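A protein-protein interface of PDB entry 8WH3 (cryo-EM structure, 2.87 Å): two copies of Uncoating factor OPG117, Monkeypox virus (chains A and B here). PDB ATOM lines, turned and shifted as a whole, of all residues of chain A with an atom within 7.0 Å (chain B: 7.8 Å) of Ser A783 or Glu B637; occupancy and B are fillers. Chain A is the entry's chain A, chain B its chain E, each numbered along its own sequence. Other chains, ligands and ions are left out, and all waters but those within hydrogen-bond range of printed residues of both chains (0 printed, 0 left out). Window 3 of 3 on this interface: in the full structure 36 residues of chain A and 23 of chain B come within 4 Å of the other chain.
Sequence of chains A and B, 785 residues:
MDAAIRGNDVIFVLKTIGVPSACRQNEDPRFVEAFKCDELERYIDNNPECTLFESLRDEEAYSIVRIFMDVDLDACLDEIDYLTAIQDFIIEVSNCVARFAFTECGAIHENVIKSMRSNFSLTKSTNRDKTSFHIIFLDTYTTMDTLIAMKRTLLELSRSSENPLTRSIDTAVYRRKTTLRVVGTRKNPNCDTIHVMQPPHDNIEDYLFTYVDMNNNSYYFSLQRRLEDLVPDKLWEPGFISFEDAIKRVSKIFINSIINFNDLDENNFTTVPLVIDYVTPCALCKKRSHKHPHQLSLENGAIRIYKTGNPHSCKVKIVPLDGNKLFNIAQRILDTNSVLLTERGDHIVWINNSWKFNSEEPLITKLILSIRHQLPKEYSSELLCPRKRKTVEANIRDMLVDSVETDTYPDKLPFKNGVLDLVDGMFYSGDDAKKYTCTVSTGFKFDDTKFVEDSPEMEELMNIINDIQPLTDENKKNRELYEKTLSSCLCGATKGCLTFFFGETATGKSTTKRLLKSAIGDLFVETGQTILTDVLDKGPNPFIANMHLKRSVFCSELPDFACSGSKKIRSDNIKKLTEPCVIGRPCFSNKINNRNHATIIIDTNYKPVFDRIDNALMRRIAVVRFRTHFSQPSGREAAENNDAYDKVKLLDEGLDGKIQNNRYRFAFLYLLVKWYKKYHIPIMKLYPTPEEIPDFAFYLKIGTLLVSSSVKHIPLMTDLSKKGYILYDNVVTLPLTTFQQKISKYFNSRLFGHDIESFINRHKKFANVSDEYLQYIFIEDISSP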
ATOM      1  N   SER A 710     -17.334 -24.691   4.662  1.00  0.00           N
ATOM      2  CA  SER A 710     -16.297 -23.664   4.642  1.00  0.00           C
ATOM      3  C   SER A 710     -15.992 -23.306   3.188  1.00  0.00           C
ATOM      4  O   SER A 710     -16.801 -23.564   2.294  1.00  0.00           O
ATOM      5  CB  SER A 710     -15.062 -24.123   5.437  1.00  0.00           C
ATOM      6  OG  SER A 710     -14.454 -25.274   4.896  1.00  0.00           O
ATOM      7  N   VAL A 711     -14.836 -22.685   2.948  1.00  0.00           N
ATOM      8  CA  VAL A 711     -14.628 -21.906   1.728  1.00  0.00           C
ATOM      9  C   VAL A 711     -14.486 -22.767   0.479  1.00  0.00           C
ATOM     10  O   VAL A 711     -15.353 -22.740  -0.400  1.00  0.00           O
ATOM     11  CB  VAL A 711     -13.397 -20.993   1.878  1.00  0.00           C
ATOM     12  N   LYS A 712     -13.409 -23.546   0.387  1.00  0.00           N
ATOM     13  CA  LYS A 712     -13.095 -24.207  -0.879  1.00  0.00           C
ATOM     14  C   LYS A 712     -12.380 -25.522  -0.589  1.00  0.00           C
ATOM     15  O   LYS A 712     -11.153 -25.551  -0.466  1.00  0.00           O
ATOM     16  CB  LYS A 712     -12.255 -23.302  -1.770  1.00  0.00           C
ATOM     17  N   LEU A 716      -8.571 -29.806  -2.272  1.00  0.00           N
ATOM     18  CA  LEU A 716      -8.285 -30.980  -1.456  1.00  0.00           C
ATOM     19  C   LEU A 716      -9.070 -32.207  -1.865  1.00  0.00           C
ATOM     20  O   LEU A 716      -8.818 -33.280  -1.306  1.00  0.00           O
ATOM     21  CB  LEU A 716      -8.530 -30.740   0.040  1.00  0.00           C
ATOM     22  CG  LEU A 716      -7.879 -29.576   0.792  1.00  0.00           C
ATOM     23  CD1 LEU A 716      -8.435 -28.192   0.450  1.00  0.00           C
ATOM     24  CD2 LEU A 716      -7.876 -29.840   2.293  1.00  0.00           C
ATOM     25  N   PHE A 778     -14.148 -34.400   9.516  1.00  0.00           N
ATOM     26  CA  PHE A 778     -13.335 -34.612  10.706  1.00  0.00           C
ATOM     27  C   PHE A 778     -12.095 -33.728  10.674  1.00  0.00           C
ATOM     28  O   PHE A 778     -11.442 -33.578   9.639  1.00  0.00           O
ATOM     29  CB  PHE A 778     -12.936 -36.083  10.823  1.00  0.00           C
ATOM     30  CG  PHE A 778     -14.040 -36.971  11.320  1.00  0.00           C
ATOM     31  CD1 PHE A 778     -15.038 -37.398  10.462  1.00  0.00           C
ATOM     32  CD2 PHE A 778     -14.079 -37.382  12.642  1.00  0.00           C
ATOM     33  CE1 PHE A 778     -16.058 -38.212  10.910  1.00  0.00           C
ATOM     34  CE2 PHE A 778     -15.097 -38.200  13.098  1.00  0.00           C
ATOM     35  CZ  PHE A 778     -16.088 -38.616  12.229  1.00  0.00           C
ATOM     36  N   ILE A 779     -11.776 -33.136  11.827  1.00  0.00           N
ATOM     37  CA  ILE A 779     -10.626 -32.240  11.914  1.00  0.00           C
ATOM     38  C   ILE A 779      -9.329 -33.015  11.709  1.00  0.00           C
ATOM     39  O   ILE A 779      -8.371 -32.505  11.114  1.00  0.00           O
ATOM     40  CB  ILE A 779     -10.645 -31.485  13.257  1.00  0.00           C
ATOM     41  CG1 ILE A 779     -11.812 -30.495  13.288  1.00  0.00           C
ATOM     42  CG2 ILE A 779      -9.329 -30.759  13.492  1.00  0.00           C
ATOM     43  CD1 ILE A 779     -11.922 -29.715  14.580  1.00  0.00           C
ATOM     44  N   GLU A 780      -9.282 -34.262  12.186  1.00  0.00           N
ATOM     45  CA  GLU A 780      -8.071 -35.067  12.049  1.00  0.00           C
ATOM     46  C   GLU A 780      -7.710 -35.283  10.585  1.00  0.00           C
ATOM     47  O   GLU A 780      -6.535 -35.210  10.210  1.00  0.00           O
ATOM     48  CB  GLU A 780      -8.253 -36.409  12.757  1.00  0.00           C
ATOM     49  CG  GLU A 780      -9.626 -37.031  12.558  1.00  0.00           C
ATOM     50  CD  GLU A 780      -9.621 -38.531  12.769  1.00  0.00           C
ATOM     51  OE1 GLU A 780      -8.830 -39.010  13.607  1.00  0.00           O
ATOM     52  OE2 GLU A 780     -10.407 -39.230  12.097  1.00  0.00           O
ATOM     53  N   ASP A 781      -8.711 -35.555   9.743  1.00  0.00           N
ATOM     54  CA  ASP A 781      -8.470 -35.626   8.306  1.00  0.00           C
ATOM     55  C   ASP A 781      -7.978 -34.281   7.790  1.00  0.00           C
ATOM     56  O   ASP A 781      -7.020 -34.214   7.010  1.00  0.00           O
ATOM     57  CB  ASP A 781      -9.762 -36.061   7.600  1.00  0.00           C
ATOM     58  CG  ASP A 781      -9.656 -36.085   6.071  1.00  0.00           C
ATOM     59  OD1 ASP A 781      -8.800 -35.416   5.458  1.00  0.00           O
ATOM     60  OD2 ASP A 781     -10.479 -36.791   5.461  1.00  0.00           O
ATOM     61  N   ILE A 782      -8.613 -33.195   8.236  1.00  0.00           N
ATOM     62  CA  ILE A 782      -8.232 -31.857   7.794  1.00  0.00           C
ATOM     63  C   ILE A 782      -6.796 -31.539   8.193  1.00  0.00           C
ATOM     64  O   ILE A 782      -6.014 -31.025   7.384  1.00  0.00           O
ATOM     65  CB  ILE A 782      -9.225 -30.826   8.360  1.00  0.00           C
ATOM     66  CG1 ILE A 782     -10.628 -31.073   7.799  1.00  0.00           C
ATOM     67  CG2 ILE A 782      -8.749 -29.413   8.100  1.00  0.00           C
ATOM     68  CD1 ILE A 782     -11.610 -29.973   8.113  1.00  0.00           C
ATOM     69  N   SER A 783      -6.425 -31.836   9.440  1.00  0.00           N
ATOM     70  CA  SER A 783      -5.071 -31.540   9.897  1.00  0.00           C
ATOM     71  C   SER A 783      -4.037 -32.367   9.144  1.00  0.00           C
ATOM     72  O   SER A 783      -2.964 -31.862   8.791  1.00  0.00           O
ATOM     73  CB  SER A 783      -4.960 -31.780  11.403  1.00  0.00           C
ATOM     74  OG  SER A 783      -3.612 -31.983  11.787  1.00  0.00           O
ATOM     75  N   SER A 784      -4.336 -33.632   8.891  1.00  0.00           N
ATOM     76  CA  SER A 784      -3.401 -34.509   8.194  1.00  0.00           C
ATOM     77  C   SER A 784      -3.325 -34.131   6.721  1.00  0.00           C
ATOM     78  O   SER A 784      -4.362 -34.092   6.045  1.00  0.00           O
ATOM     79  CB  SER A 784      -3.828 -35.966   8.346  1.00  0.00           C
ATOM     80  OG  SER A 784      -4.978 -36.244   7.565  1.00  0.00           O
ATOM     81  N   PRO A 785      -2.132 -33.842   6.178  1.00  0.00           N
ATOM     82  CA  PRO A 785      -1.957 -33.479   4.766  1.00  0.00           C
ATOM     83  C   PRO A 785      -2.360 -34.602   3.815  1.00  0.00           C
ATOM     84  O   PRO A 785      -3.476 -34.574   3.295  1.00  0.00           O
ATOM     85  CB  PRO A 785      -0.453 -33.194   4.660  1.00  0.00           C
ATOM     86  CG  PRO A 785      -0.013 -32.911   6.058  1.00  0.00           C
ATOM     87  CD  PRO A 785      -0.864 -33.783   6.923  1.00  0.00           C
ATOM     88  N   SER B 631     -11.983 -15.490   9.425  1.00  0.00           N
ATOM     89  CA  SER B 631     -11.802 -16.632  10.311  1.00  0.00           C
ATOM     90  C   SER B 631     -10.493 -16.478  11.071  1.00  0.00           C
ATOM     91  O   SER B 631      -9.620 -15.692  10.699  1.00  0.00           O
ATOM     92  CB  SER B 631     -11.823 -17.950   9.531  1.00  0.00           C
ATOM     93  OG  SER B 631     -11.116 -17.835   8.308  1.00  0.00           O
ATOM     94  N   GLN B 632     -10.374 -17.250  12.154  1.00  0.00           N
ATOM     95  CA  GLN B 632      -9.156 -17.315  12.944  1.00  0.00           C
ATOM     96  C   GLN B 632      -8.140 -18.244  12.280  1.00  0.00           C
ATOM     97  O   GLN B 632      -8.518 -19.182  11.574  1.00  0.00           O
ATOM     98  CB  GLN B 632      -9.462 -17.804  14.358  1.00  0.00           C
ATOM     99  CG  GLN B 632     -10.520 -16.989  15.093  1.00  0.00           C
ATOM    100  CD  GLN B 632     -11.931 -17.481  14.836  1.00  0.00           C
ATOM    101  OE1 GLN B 632     -12.299 -18.584  15.242  1.00  0.00           O
ATOM    102  NE2 GLN B 632     -12.730 -16.663  14.162  1.00  0.00           N
ATOM    103  N   PRO B 633      -6.842 -17.995  12.484  1.00  0.00           N
ATOM    104  CA  PRO B 633      -5.825 -18.824  11.812  1.00  0.00           C
ATOM    105  C   PRO B 633      -5.895 -20.301  12.162  1.00  0.00           C
ATOM    106  O   PRO B 633      -5.625 -21.143  11.295  1.00  0.00           O
ATOM    107  CB  PRO B 633      -4.496 -18.205  12.271  1.00  0.00           C
ATOM    108  CG  PRO B 633      -4.830 -16.871  12.823  1.00  0.00           C
ATOM    109  CD  PRO B 633      -6.255 -16.891  13.261  1.00  0.00           C
ATOM    110  N   SER B 634      -6.239 -20.647  13.406  1.00  0.00           N
ATOM    111  CA  SER B 634      -6.311 -22.055  13.785  1.00  0.00           C
ATOM    112  C   SER B 634      -7.382 -22.782  12.982  1.00  0.00           C
ATOM    113  O   SER B 634      -7.148 -23.877  12.458  1.00  0.00           O
ATOM    114  CB  SER B 634      -6.580 -22.182  15.285  1.00  0.00           C
ATOM    115  OG  SER B 634      -6.485 -23.532  15.706  1.00  0.00           O
ATOM    116  N   GLY B 635      -8.562 -22.183  12.871  1.00  0.00           N
ATOM    117  CA  GLY B 635      -9.628 -22.718  12.057  1.00  0.00           C
ATOM    118  C   GLY B 635      -9.603 -22.299  10.607  1.00  0.00           C
ATOM    119  O   GLY B 635     -10.469 -22.735   9.843  1.00  0.00           O
ATOM    120  N   ARG B 636      -8.629 -21.478  10.199  1.00  0.00           N
ATOM    121  CA  ARG B 636      -8.591 -20.977   8.827  1.00  0.00           C
ATOM    122  C   ARG B 636      -8.507 -22.114   7.819  1.00  0.00           C
ATOM    123  O   ARG B 636      -9.192 -22.095   6.789  1.00  0.00           O
ATOM    124  CB  ARG B 636      -7.412 -20.021   8.648  1.00  0.00           C
ATOM    125  CG  ARG B 636      -7.012 -19.809   7.196  1.00  0.00           C
ATOM    126  CD  ARG B 636      -6.110 -18.600   7.012  1.00  0.00           C
ATOM    127  NE  ARG B 636      -6.139 -18.128   5.632  1.00  0.00           N
ATOM    128  CZ  ARG B 636      -6.572 -16.934   5.253  1.00  0.00           C
ATOM    129  NH1 ARG B 636      -7.021 -16.051   6.129  1.00  0.00           N
ATOM    130  NH2 ARG B 636      -6.556 -16.619   3.961  1.00  0.00           N
ATOM    131  N   GLU B 637      -7.672 -23.113   8.095  1.00  0.00           N
ATOM    132  CA  GLU B 637      -7.624 -24.296   7.244  1.00  0.00           C
ATOM    133  C   GLU B 637      -8.973 -25.008   7.232  1.00  0.00           C
ATOM    134  O   GLU B 637      -9.503 -25.360   6.167  1.00  0.00           O
ATOM    135  CB  GLU B 637      -6.507 -25.217   7.735  1.00  0.00           C
ATOM    136  CG  GLU B 637      -6.570 -26.639   7.235  1.00  0.00           C
ATOM    137  CD  GLU B 637      -5.461 -27.494   7.815  1.00  0.00           C
ATOM    138  OE1 GLU B 637      -4.285 -27.252   7.474  1.00  0.00           O
ATOM    139  OE2 GLU B 637      -5.763 -28.400   8.619  1.00  0.00           O
ATOM    140  N   ALA B 638      -9.566 -25.194   8.415  1.00  0.00           N
ATOM    141  CA  ALA B 638     -10.905 -25.766   8.492  1.00  0.00           C
ATOM    142  C   ALA B 638     -11.955 -24.802   7.957  1.00  0.00           C
ATOM    143  O   ALA B 638     -13.048 -25.233   7.570  1.00  0.00           O
ATOM    144  CB  ALA B 638     -11.227 -26.159   9.934  1.00  0.00           C
ATOM    145  N   ALA B 639     -11.651 -23.505   7.935  1.00  0.00           N
ATOM    146  CA  ALA B 639     -12.518 -22.516   7.309  1.00  0.00           C
ATOM    147  C   ALA B 639     -12.310 -22.427   5.806  1.00  0.00           C
ATOM    148  O   ALA B 639     -12.999 -21.645   5.143  1.00  0.00           O
ATOM    149  CB  ALA B 639     -12.303 -21.138   7.940  1.00  0.00           C
ATOM    150  N   GLU B 640     -11.372 -23.198   5.259  1.00  0.00           N
ATOM    151  CA  GLU B 640     -11.173 -23.282   3.818  1.00  0.00           C
ATOM    152  C   GLU B 640     -11.256 -24.709   3.294  1.00  0.00           C
ATOM    153  O   GLU B 640     -10.953 -24.935   2.120  1.00  0.00           O
ATOM    154  CB  GLU B 640      -9.824 -22.670   3.424  1.00  0.00           C
ATOM    155  CG  GLU B 640      -9.824 -21.158   3.290  1.00  0.00           C
ATOM    156  CD  GLU B 640      -9.026 -20.686   2.088  1.00  0.00           C
ATOM    157  OE1 GLU B 640      -7.780 -20.760   2.129  1.00  0.00           O
ATOM    158  OE2 GLU B 640      -9.648 -20.247   1.097  1.00  0.00           O
ATOM    159  N   ASN B 641     -11.654 -25.682   4.118  1.00  0.00           N
ATOM    160  CA  ASN B 641     -11.712 -27.045   3.595  1.00  0.00           C
ATOM    161  C   ASN B 641     -13.128 -27.599   3.450  1.00  0.00           C
ATOM    162  O   ASN B 641     -13.359 -28.781   3.717  1.00  0.00           O
ATOM    163  CB  ASN B 641     -10.894 -27.995   4.473  1.00  0.00           C
ATOM    164  CG  ASN B 641      -9.415 -27.684   4.434  1.00  0.00           C
ATOM    165  OD1 ASN B 641      -8.683 -27.984   5.374  1.00  0.00           O
ATOM    166  ND2 ASN B 641      -8.982 -27.002   3.383  1.00  0.00           N
ATOM    167  N   ASN B 642     -14.076 -26.774   3.021  1.00  0.00           N
ATOM    168  CA  ASN B 642     -15.415 -27.257   2.673  1.00  0.00           C
ATOM    169  C   ASN B 642     -15.986 -26.314   1.614  1.00  0.00           C
ATOM    170  O   ASN B 642     -15.236 -25.633   0.909  1.00  0.00           O
ATOM    171  CB  ASN B 642     -16.292 -27.407   3.927  1.00  0.00           C
ATOM    172  CG  ASN B 642     -17.239 -28.586   3.841  1.00  0.00           C
ATOM    173  OD1 ASN B 642     -17.616 -29.016   2.752  1.00  0.00           O
ATOM    174  ND2 ASN B 642     -17.639 -29.108   4.995  1.00  0.00           N
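OG of Ser A710 lies within hydrogen-bond range of O of Ala B638 (3.0 Å).
The side-chain hydroxyl (OG) of Ser A710 is in hydrogen-bond range of the backbone NH (N) of Asn B641, at 2.9 Å.
The backbone NH (N) of Asn B642 sits at hydrogen-bond distance from the side-chain hydroxyl (OG) of Ser A710 (2.4 Å).
N of Val A711 sits at hydrogen-bond distance from O of Ala B639, at 3.0 Å.
N of Lys A712 sits close to O of Glu B640.
The backbone NH (N) of Lys A712 lies within hydrogen-bond range of the backbone carbonyl oxygen (O) of Asn B642.
O of Val A711 lies close to O of Asn B642 (3.2 Å).
OE2 of Glu B637 lies close to O of Ile A782, at 2.9 Å.
O of Glu B637 sits close to OD1 of Asn B641.
Among the printed residues, pairs that only touch across the chains: Ser A710 with Ala B639 (3.2 Å), Ser A710 with Glu B640 (3.6 Å), Val A711 with Glu B640 (3.7 Å), Leu A716 with Asn B641 (3.2 Å), Ile A782 with Asn B641 (3.1 Å) and Ser A783 with Glu B637 (3.5 Å).
Printed residues of chain B within 4 Å of Lys A712: Glu B640 (2.7 Å) and Asn B642 (2.8 Å).
Printed residues of chain B within 4 Å of Ser A783: Glu B637 (3.5 Å).
Pro B633 touches none of the printed residues of chain A.
Glu B637 touches just these residues of chain A: Ile A782 and Ser A783.
Of the printed residues of chain A, Glu B640 touches Ser A710, Val A711 and Lys A712.
Printed residues of chain A within 4 Å of Asn B642: Ser A710 (2.4 Å), Val A711 (3.0 Å) and Lys A712 (2.8 Å).
The nearest residue of chain B that does not touch Ser A783 is Asn B641 (6.0 Å).
The nearest residue of chain A that does not touch Glu B637 is Ser A710 (5.1 Å).
The nearest printed residue of chain A that does not touch Ala B638 is Ile A782 (4.2 Å).
Printed residues of chain A that touch a printed residue of chain B: Ser A710, Val A711, Lys A712, Leu A716, Ile A782 and Ser A783.
No position is printed for both chains.
Of the 14 pairs that touch across the chains among the printed residues, none has its exchanged pair printed and touching as well.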
